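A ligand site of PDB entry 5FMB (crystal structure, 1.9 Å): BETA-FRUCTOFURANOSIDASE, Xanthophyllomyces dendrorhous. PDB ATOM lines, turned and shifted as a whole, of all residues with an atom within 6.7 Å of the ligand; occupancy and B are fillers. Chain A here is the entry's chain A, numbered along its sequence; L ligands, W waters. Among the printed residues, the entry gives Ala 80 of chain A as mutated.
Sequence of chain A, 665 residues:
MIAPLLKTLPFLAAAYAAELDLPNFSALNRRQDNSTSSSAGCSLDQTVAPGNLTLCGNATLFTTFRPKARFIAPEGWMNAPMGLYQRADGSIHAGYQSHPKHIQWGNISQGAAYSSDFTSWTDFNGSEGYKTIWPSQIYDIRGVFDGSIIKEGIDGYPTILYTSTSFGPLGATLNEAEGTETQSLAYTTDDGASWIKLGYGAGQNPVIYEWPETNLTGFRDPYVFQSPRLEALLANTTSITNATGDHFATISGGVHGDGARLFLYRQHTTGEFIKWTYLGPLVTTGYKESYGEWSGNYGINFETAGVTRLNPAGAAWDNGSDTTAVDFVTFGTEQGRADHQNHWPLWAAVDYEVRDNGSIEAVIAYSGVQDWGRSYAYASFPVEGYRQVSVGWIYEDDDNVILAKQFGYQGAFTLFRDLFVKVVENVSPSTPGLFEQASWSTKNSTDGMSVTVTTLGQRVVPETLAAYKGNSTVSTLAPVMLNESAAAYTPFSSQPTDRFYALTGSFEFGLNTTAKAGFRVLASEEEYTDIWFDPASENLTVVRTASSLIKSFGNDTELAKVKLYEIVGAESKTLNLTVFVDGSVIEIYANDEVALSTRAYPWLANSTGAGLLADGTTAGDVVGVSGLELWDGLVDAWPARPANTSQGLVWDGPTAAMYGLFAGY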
ATOM      1  N   TRP A  77     -18.547   4.117  21.962  1.00  0.00           N
ATOM      2  CA  TRP A  77     -17.419   4.888  21.503  1.00  0.00           C
ATOM      3  C   TRP A  77     -17.707   5.535  20.145  1.00  0.00           C
ATOM      4  O   TRP A  77     -18.188   4.867  19.237  1.00  0.00           O
ATOM      5  CB  TRP A  77     -16.192   3.979  21.365  1.00  0.00           C
ATOM      6  CG  TRP A  77     -15.058   4.677  20.688  1.00  0.00           C
ATOM      7  CD1 TRP A  77     -14.832   4.743  19.348  1.00  0.00           C
ATOM      8  CD2 TRP A  77     -14.053   5.480  21.307  1.00  0.00           C
ATOM      9  NE1 TRP A  77     -13.748   5.538  19.089  1.00  0.00           N
ATOM     10  CE2 TRP A  77     -13.239   5.990  20.279  1.00  0.00           C
ATOM     11  CE3 TRP A  77     -13.749   5.805  22.644  1.00  0.00           C
ATOM     12  CZ2 TRP A  77     -12.138   6.810  20.539  1.00  0.00           C
ATOM     13  CZ3 TRP A  77     -12.668   6.625  22.899  1.00  0.00           C
ATOM     14  CH2 TRP A  77     -11.870   7.127  21.855  1.00  0.00           C
ATOM     15  N   ASN A  79     -15.535   8.493  17.422  1.00  0.00           N
ATOM     16  CA  ASN A  79     -14.505   9.487  17.175  1.00  0.00           C
ATOM     17  C   ASN A  79     -14.792  10.305  15.894  1.00  0.00           C
ATOM     18  O   ASN A  79     -15.841  10.964  15.827  1.00  0.00           O
ATOM     19  CB  ASN A  79     -13.055   8.926  17.364  1.00  0.00           C
ATOM     20  CG  ASN A  79     -12.693   7.750  16.476  1.00  0.00           C
ATOM     21  OD1 ASN A  79     -13.232   6.648  16.590  1.00  0.00           O
ATOM     22  ND2 ASN A  79     -11.705   7.953  15.610  1.00  0.00           N
ATOM     23  N   ALA A  80     -13.904  10.289  14.898  1.00  0.00           N
ATOM     24  CA  ALA A  80     -13.914  11.237  13.781  1.00  0.00           C
ATOM     25  C   ALA A  80     -15.212  11.254  12.985  1.00  0.00           C
ATOM     26  O   ALA A  80     -15.752  10.206  12.678  1.00  0.00           O
ATOM     27  CB  ALA A  80     -12.767  10.912  12.823  1.00  0.00           C
ATOM     28  N   GLN A  97     -16.847   7.550  12.974  1.00  0.00           N
ATOM     29  CA  GLN A  97     -16.120   6.393  13.462  1.00  0.00           C
ATOM     30  C   GLN A  97     -16.839   5.934  14.752  1.00  0.00           C
ATOM     31  O   GLN A  97     -17.059   6.751  15.649  1.00  0.00           O
ATOM     32  CB  GLN A  97     -14.673   6.759  13.743  1.00  0.00           C
ATOM     33  CG  GLN A  97     -13.877   7.097  12.478  1.00  0.00           C
ATOM     34  CD  GLN A  97     -13.439   5.855  11.728  1.00  0.00           C
ATOM     35  OE1 GLN A  97     -12.422   5.271  12.068  1.00  0.00           O
ATOM     36  NE2 GLN A  97     -14.212   5.443  10.712  1.00  0.00           N
ATOM     37  N   TRP A 105     -11.900   2.492  21.417  1.00  0.00           N
ATOM     38  CA  TRP A 105     -11.866   2.282  19.978  1.00  0.00           C
ATOM     39  C   TRP A 105     -11.698   0.804  19.583  1.00  0.00           C
ATOM     40  O   TRP A 105     -11.096   0.017  20.306  1.00  0.00           O
ATOM     41  CB  TRP A 105     -10.696   3.104  19.443  1.00  0.00           C
ATOM     42  CG  TRP A 105     -10.436   3.138  17.972  1.00  0.00           C
ATOM     43  CD1 TRP A 105     -10.849   4.084  17.081  1.00  0.00           C
ATOM     44  CD2 TRP A 105      -9.589   2.240  17.242  1.00  0.00           C
ATOM     45  NE1 TRP A 105     -10.348   3.805  15.830  1.00  0.00           N
ATOM     46  CE2 TRP A 105      -9.579   2.683  15.895  1.00  0.00           C
ATOM     47  CE3 TRP A 105      -8.861   1.093  17.575  1.00  0.00           C
ATOM     48  CZ2 TRP A 105      -8.848   2.036  14.907  1.00  0.00           C
ATOM     49  CZ3 TRP A 105      -8.142   0.434  16.592  1.00  0.00           C
ATOM     50  CH2 TRP A 105      -8.136   0.915  15.260  1.00  0.00           C
ATOM     51  N   ILE A 108     -13.573  -0.557  13.987  1.00  0.00           N
ATOM     52  CA  ILE A 108     -14.117   0.762  13.779  1.00  0.00           C
ATOM     53  C   ILE A 108     -14.973   0.775  12.496  1.00  0.00           C
ATOM     54  O   ILE A 108     -14.599   0.199  11.485  1.00  0.00           O
ATOM     55  CB  ILE A 108     -13.043   1.865  13.872  1.00  0.00           C
ATOM     56  CG1 ILE A 108     -13.688   3.200  14.309  1.00  0.00           C
ATOM     57  CG2 ILE A 108     -12.278   2.016  12.563  1.00  0.00           C
ATOM     58  CD1 ILE A 108     -14.152   3.242  15.767  1.00  0.00           C
ATOM     59  N   VAL A 144     -12.820   0.047   9.332  1.00  0.00           N
ATOM     60  CA  VAL A 144     -13.271   0.978   8.313  1.00  0.00           C
ATOM     61  C   VAL A 144     -12.970   2.371   8.854  1.00  0.00           C
ATOM     62  O   VAL A 144     -13.740   2.922   9.641  1.00  0.00           O
ATOM     63  CB  VAL A 144     -14.776   0.803   8.021  1.00  0.00           C
ATOM     64  CG1 VAL A 144     -15.304   1.890   7.097  1.00  0.00           C
ATOM     65  CG2 VAL A 144     -15.028  -0.571   7.412  1.00  0.00           C
ATOM     66  N   PHE A 145     -11.833   2.906   8.439  1.00  0.00           N
ATOM     67  CA  PHE A 145     -11.336   4.205   8.905  1.00  0.00           C
ATOM     68  C   PHE A 145     -12.053   5.336   8.145  1.00  0.00           C
ATOM     69  O   PHE A 145     -13.002   5.086   7.397  1.00  0.00           O
ATOM     70  CB  PHE A 145      -9.806   4.279   8.720  1.00  0.00           C
ATOM     71  CG  PHE A 145      -8.988   3.615   9.800  1.00  0.00           C
ATOM     72  CD1 PHE A 145      -9.417   2.487  10.471  1.00  0.00           C
ATOM     73  CD2 PHE A 145      -7.702   4.089  10.063  1.00  0.00           C
ATOM     74  CE1 PHE A 145      -8.616   1.870  11.417  1.00  0.00           C
ATOM     75  CE2 PHE A 145      -6.888   3.473  11.002  1.00  0.00           C
ATOM     76  CZ  PHE A 145      -7.350   2.363  11.678  1.00  0.00           C
ATOM     77  N   ASP A 146     -11.612   6.564   8.357  1.00  0.00           N
ATOM     78  CA  ASP A 146     -12.206   7.770   7.755  1.00  0.00           C
ATOM     79  C   ASP A 146     -12.282   7.659   6.226  1.00  0.00           C
ATOM     80  O   ASP A 146     -11.456   7.012   5.577  1.00  0.00           O
ATOM     81  CB  ASP A 146     -11.363   8.987   8.167  1.00  0.00           C
ATOM     82  CG  ASP A 146     -11.973  10.332   7.820  1.00  0.00           C
ATOM     83  OD1 ASP A 146     -13.183  10.467   7.545  1.00  0.00           O
ATOM     84  OD2 ASP A 146     -11.177  11.321   7.865  1.00  0.00           O
ATOM     85  N   GLY A 147     -13.303   8.300   5.673  1.00  0.00           N
ATOM     86  CA  GLY A 147     -13.473   8.417   4.223  1.00  0.00           C
ATOM     87  C   GLY A 147     -14.348   9.609   3.899  1.00  0.00           C
ATOM     88  O   GLY A 147     -14.959  10.192   4.786  1.00  0.00           O
ATOM     89  N   THR A 163     -10.444   4.644   4.076  1.00  0.00           N
ATOM     90  CA  THR A 163      -9.289   3.834   4.402  1.00  0.00           C
ATOM     91  C   THR A 163      -9.723   2.471   4.936  1.00  0.00           C
ATOM     92  O   THR A 163     -10.335   2.364   6.021  1.00  0.00           O
ATOM     93  CB  THR A 163      -8.349   4.549   5.378  1.00  0.00           C
ATOM     94  OG1 THR A 163      -7.843   5.733   4.766  1.00  0.00           O
ATOM     95  CG2 THR A 163      -7.186   3.629   5.785  1.00  0.00           C
ATOM     96  N   GLU A 181      -2.776  -0.239   5.473  1.00  0.00           N
ATOM     97  CA  GLU A 181      -3.746   0.798   5.155  1.00  0.00           C
ATOM     98  C   GLU A 181      -3.860   0.944   3.651  1.00  0.00           C
ATOM     99  O   GLU A 181      -2.877   1.261   2.997  1.00  0.00           O
ATOM    100  CB  GLU A 181      -3.319   2.127   5.763  1.00  0.00           C
ATOM    101  CG  GLU A 181      -3.216   2.121   7.273  1.00  0.00           C
ATOM    102  CD  GLU A 181      -2.915   3.505   7.812  1.00  0.00           C
ATOM    103  OE1 GLU A 181      -1.736   3.937   7.739  1.00  0.00           O
ATOM    104  OE2 GLU A 181      -3.838   4.156   8.321  1.00  0.00           O
ATOM    105  N   ARG A 220      -3.686   7.352   5.099  1.00  0.00           N
ATOM    106  CA  ARG A 220      -5.125   7.260   5.368  1.00  0.00           C
ATOM    107  C   ARG A 220      -5.886   8.567   5.195  1.00  0.00           C
ATOM    108  O   ARG A 220      -5.295   9.635   4.965  1.00  0.00           O
ATOM    109  CB  ARG A 220      -5.342   6.709   6.791  1.00  0.00           C
ATOM    110  CG  ARG A 220      -4.704   7.505   7.926  1.00  0.00           C
ATOM    111  CD  ARG A 220      -5.224   7.013   9.286  1.00  0.00           C
ATOM    112  NE  ARG A 220      -4.422   7.526  10.386  1.00  0.00           N
ATOM    113  CZ  ARG A 220      -3.201   7.078  10.737  1.00  0.00           C
ATOM    114  NH1 ARG A 220      -2.628   6.083  10.066  1.00  0.00           N
ATOM    115  NH2 ARG A 220      -2.549   7.639  11.740  1.00  0.00           N
ATOM    116  N   ASP A 221      -7.205   8.446   5.326  1.00  0.00           N
ATOM    117  CA  ASP A 221      -8.131   9.558   5.384  1.00  0.00           C
ATOM    118  C   ASP A 221      -8.246  10.259   4.039  1.00  0.00           C
ATOM    119  O   ASP A 221      -7.978  11.471   3.930  1.00  0.00           O
ATOM    120  CB  ASP A 221      -7.761  10.537   6.514  1.00  0.00           C
ATOM    121  CG  ASP A 221      -7.610   9.834   7.880  1.00  0.00           C
ATOM    122  OD1 ASP A 221      -8.101   8.702   8.012  1.00  0.00           O
ATOM    123  OD2 ASP A 221      -6.936  10.420   8.766  1.00  0.00           O
ATOM    124  N   SER A 252      -3.471  11.426   3.881  1.00  0.00           N
ATOM    125  CA  SER A 252      -2.723  11.986   4.993  1.00  0.00           C
ATOM    126  C   SER A 252      -1.686  11.006   5.525  1.00  0.00           C
ATOM    127  O   SER A 252      -1.966   9.812   5.716  1.00  0.00           O
ATOM    128  CB  SER A 252      -3.689  12.376   6.123  1.00  0.00           C
ATOM    129  OG  SER A 252      -4.640  13.326   5.694  1.00  0.00           O
ATOM    130  N   PHE A 302       0.288  13.567   9.556  1.00  0.00           N
ATOM    131  CA  PHE A 302      -1.017  14.188   9.404  1.00  0.00           C
ATOM    132  C   PHE A 302      -2.132  13.155   9.466  1.00  0.00           C
ATOM    133  O   PHE A 302      -1.972  12.016   9.021  1.00  0.00           O
ATOM    134  CB  PHE A 302      -1.182  14.929   8.051  1.00  0.00           C
ATOM    135  CG  PHE A 302      -0.326  16.170   7.874  1.00  0.00           C
ATOM    136  CD1 PHE A 302       0.051  16.985   8.942  1.00  0.00           C
ATOM    137  CD2 PHE A 302       0.068  16.536   6.599  1.00  0.00           C
ATOM    138  CE1 PHE A 302       0.823  18.117   8.728  1.00  0.00           C
ATOM    139  CE2 PHE A 302       0.843  17.679   6.377  1.00  0.00           C
ATOM    140  CZ  PHE A 302       1.211  18.465   7.439  1.00  0.00           C
ATOM    141  N   GLU A 303      -3.272  13.597   9.972  1.00  0.00           N
ATOM    142  CA  GLU A 303      -4.521  12.836   9.920  1.00  0.00           C
ATOM    143  C   GLU A 303      -5.661  13.759   9.499  1.00  0.00           C
ATOM    144  O   GLU A 303      -5.635  14.968   9.753  1.00  0.00           O
ATOM    145  CB  GLU A 303      -4.844  12.210  11.273  1.00  0.00           C
ATOM    146  CG  GLU A 303      -3.805  11.215  11.761  1.00  0.00           C
ATOM    147  CD  GLU A 303      -4.189  10.562  13.074  1.00  0.00           C
ATOM    148  OE1 GLU A 303      -4.325  11.287  14.085  1.00  0.00           O
ATOM    149  OE2 GLU A 303      -4.333   9.313  13.106  1.00  0.00           O
ATOM    150  N   THR A 304      -6.676  13.147   8.882  1.00  0.00           N
ATOM    151  CA  THR A 304      -7.921  13.794   8.468  1.00  0.00           C
ATOM    152  C   THR A 304      -7.733  15.129   7.770  1.00  0.00           C
ATOM    153  O   THR A 304      -8.496  16.063   7.995  1.00  0.00           O
ATOM    154  CB  THR A 304      -8.960  13.933   9.639  1.00  0.00           C
ATOM    155  OG1 THR A 304      -8.612  15.015  10.506  1.00  0.00           O
ATOM    156  CG2 THR A 304      -9.059  12.660  10.432  1.00  0.00           C
ATOM    157  N   GLU A 334       0.032  14.701  14.715  1.00  0.00           N
ATOM    158  CA  GLU A 334       0.312  13.813  15.830  1.00  0.00           C
ATOM    159  C   GLU A 334       1.752  13.959  16.330  1.00  0.00           C
ATOM    160  O   GLU A 334       2.668  14.170  15.539  1.00  0.00           O
ATOM    161  CB  GLU A 334       0.193  12.348  15.422  1.00  0.00           C
ATOM    162  CG  GLU A 334      -1.005  11.978  14.601  1.00  0.00           C
ATOM    163  CD  GLU A 334      -1.227  10.481  14.652  1.00  0.00           C
ATOM    164  OE1 GLU A 334      -1.839  10.031  15.658  1.00  0.00           O
ATOM    165  OE2 GLU A 334      -0.772   9.776  13.728  1.00  0.00           O
ATOM    166  N   HIS A 343      -2.291  15.753  19.978  1.00  0.00           N
ATOM    167  CA  HIS A 343      -3.027  16.085  18.749  1.00  0.00           C
ATOM    168  C   HIS A 343      -3.359  17.565  18.600  1.00  0.00           C
ATOM    169  O   HIS A 343      -3.970  18.159  19.487  1.00  0.00           O
ATOM    170  CB  HIS A 343      -4.341  15.316  18.742  1.00  0.00           C
ATOM    171  CG  HIS A 343      -4.189  13.876  18.368  1.00  0.00           C
ATOM    172  ND1 HIS A 343      -5.053  12.894  18.807  1.00  0.00           N
ATOM    173  CD2 HIS A 343      -3.276  13.249  17.588  1.00  0.00           C
ATOM    174  CE1 HIS A 343      -4.675  11.727  18.322  1.00  0.00           C
ATOM    175  NE2 HIS A 343      -3.597  11.917  17.583  1.00  0.00           N
ATOM    176  N   TYR A 376     -10.464  17.338  17.643  1.00  0.00           N
ATOM    177  CA  TYR A 376      -9.557  16.813  16.615  1.00  0.00           C
ATOM    178  C   TYR A 376     -10.418  16.229  15.500  1.00  0.00           C
ATOM    179  O   TYR A 376     -11.635  16.121  15.639  1.00  0.00           O
ATOM    180  CB  TYR A 376      -8.704  15.696  17.214  1.00  0.00           C
ATOM    181  CG  TYR A 376      -7.514  15.243  16.407  1.00  0.00           C
ATOM    182  CD1 TYR A 376      -6.482  16.127  16.073  1.00  0.00           C
ATOM    183  CD2 TYR A 376      -7.387  13.906  16.010  1.00  0.00           C
ATOM    184  CE1 TYR A 376      -5.363  15.698  15.376  1.00  0.00           C
ATOM    185  CE2 TYR A 376      -6.278  13.477  15.309  1.00  0.00           C
ATOM    186  CZ  TYR A 376      -5.268  14.369  14.981  1.00  0.00           C
ATOM    187  OH  TYR A 376      -4.162  13.949  14.292  1.00  0.00           O
ATOM    188  N   ALA A 377      -9.776  15.878  14.382  1.00  0.00           N
ATOM    189  CA  ALA A 377     -10.417  15.137  13.295  1.00  0.00           C
ATOM    190  C   ALA A 377     -11.514  15.959  12.642  1.00  0.00           C
ATOM    191  O   ALA A 377     -12.602  15.478  12.410  1.00  0.00           O
ATOM    192  CB  ALA A 377     -10.953  13.796  13.784  1.00  0.00           C
ATOM    193  N   TRP A 393     -14.503  16.330  16.255  1.00  0.00           N
ATOM    194  CA  TRP A 393     -14.803  15.407  17.334  1.00  0.00           C
ATOM    195  C   TRP A 393     -14.241  15.957  18.635  1.00  0.00           C
ATOM    196  O   TRP A 393     -13.064  16.313  18.686  1.00  0.00           O
ATOM    197  CB  TRP A 393     -14.199  14.046  17.009  1.00  0.00           C
ATOM    198  CG  TRP A 393     -13.865  13.136  18.155  1.00  0.00           C
ATOM    199  CD1 TRP A 393     -14.737  12.580  19.047  1.00  0.00           C
ATOM    200  CD2 TRP A 393     -12.580  12.596  18.458  1.00  0.00           C
ATOM    201  NE1 TRP A 393     -14.060  11.746  19.919  1.00  0.00           N
ATOM    202  CE2 TRP A 393     -12.733  11.735  19.564  1.00  0.00           C
ATOM    203  CE3 TRP A 393     -11.313  12.769  17.903  1.00  0.00           C
ATOM    204  CZ2 TRP A 393     -11.662  11.044  20.124  1.00  0.00           C
ATOM    205  CZ3 TRP A 393     -10.242  12.078  18.462  1.00  0.00           C
ATOM    206  CH2 TRP A 393     -10.424  11.237  19.563  1.00  0.00           C
HETATM  207  C1  LIG L   1      -8.080  10.496  13.607  1.00  0.00           C
HETATM  208  C2  LIG L   1      -8.088   9.053  13.054  1.00  0.00           C
HETATM  209  C3  LIG L   1      -8.052   8.994  11.532  1.00  0.00           C
HETATM  210  C4  LIG L   1      -8.532   7.569  11.272  1.00  0.00           C
HETATM  211  C5  LIG L   1      -9.547   7.353  12.391  1.00  0.00           C
HETATM  212  C6  LIG L   1      -9.527   5.950  12.968  1.00  0.00           C
HETATM  213  O1  LIG L   1      -8.073  10.475  15.047  1.00  0.00           O
HETATM  214  O2  LIG L   1      -6.970   8.346  13.593  1.00  0.00           O
HETATM  215  O3  LIG L   1      -6.766   9.304  11.021  1.00  0.00           O
HETATM  216  O4  LIG L   1      -9.152   7.387   9.995  1.00  0.00           O
HETATM  217  O5  LIG L   1      -9.247   8.325  13.397  1.00  0.00           O
HETATM  218  O6  LIG L   1     -10.645   5.770  13.855  1.00  0.00           O
HETATM  219  O   HOH W   1     -10.556  10.663  15.618  1.00  0.00           O
HETATM  220  O   HOH W   2      -5.755   9.911  16.053  1.00  0.00           O
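The side-chain carboxylate (OD2) of Asp 221 sits at hydrogen-bond distance from an oxygen (O3) of the ligand (2.5 Å). The side-chain amide oxygen (OE1) of Gln 97 lies within hydrogen-bond range of an oxygen (O6) of the ligand (2.6 Å). The indole nitrogen of Trp 105 is in hydrogen-bond range of an oxygen (O6) of the ligand. An oxygen (O2) of the ligand sits at hydrogen-bond distance from the side-chain carboxylate (OE2) of Glu 303 (2.9 Å). The side-chain amide nitrogen of Asn 79 is in hydrogen-bond range of an oxygen (O6) of the ligand, at 3.0 Å. An oxygen (O3) of the ligand lies within hydrogen-bond range of the guanidinium group (NE) of Arg 220, at 3.0 Å. O4 of the ligand sits at hydrogen-bond distance from N of Asp 146, at 3.1 Å.
The side-chain carboxylate (OD2) of Asp 221 lies within hydrogen-bond range of the backbone NH (N) of Thr 304 (2.7 Å). The backbone carbonyl oxygen (O) of Gln 97 is in hydrogen-bond range of the backbone NH (N) of Asn 79, 2.9 Å away. The backbone NH (N) of Gln 97 lies within hydrogen-bond range of the backbone carbonyl oxygen (O) of Ala 80 (2.9 Å). The side-chain amide nitrogen (NE2) of Gln 97 sits at hydrogen-bond distance from the backbone carbonyl oxygen (O) of Val 144, 2.8 Å away. OH of Tyr 376 is in hydrogen-bond range of OE1 of Glu 303. OD1 of Asn 79 sits at hydrogen-bond distance from NE1 of Trp 77, at 2.8 Å. The side-chain carboxylate (OE2) of Glu 334 is in salt-bridge range of the guanidinium group (NH2) of Arg 220 (3.4 Å). O of Arg 220 is in hydrogen-bond range of N of Ser 252.
Merely in contact with the ligand: Phe 145 (3.4 Å), Tyr 376 (3.5 Å) and Thr 304 (3.96 Å). Hydrophobic or aromatic side chains that line the ligand: Trp 105, Phe 145 and Tyr 376. Within 4 Å of the ligand: Asn 79, Gln 97, Trp 105, Phe 145, Asp 146, Arg 220, Asp 221, Glu 303, Thr 304 and Tyr 376.
Water W1 lies within hydrogen-bond range of an oxygen (O1) of the ligand, the side-chain amide nitrogen (ND2) of Asn 79 and the backbone NH (N) of Ala 80. Water W2 lies within hydrogen-bond range of an oxygen (O1) of the ligand, the side-chain carboxylate (OE1) of Glu 303 and a ring nitrogen (NE2) of His 343.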
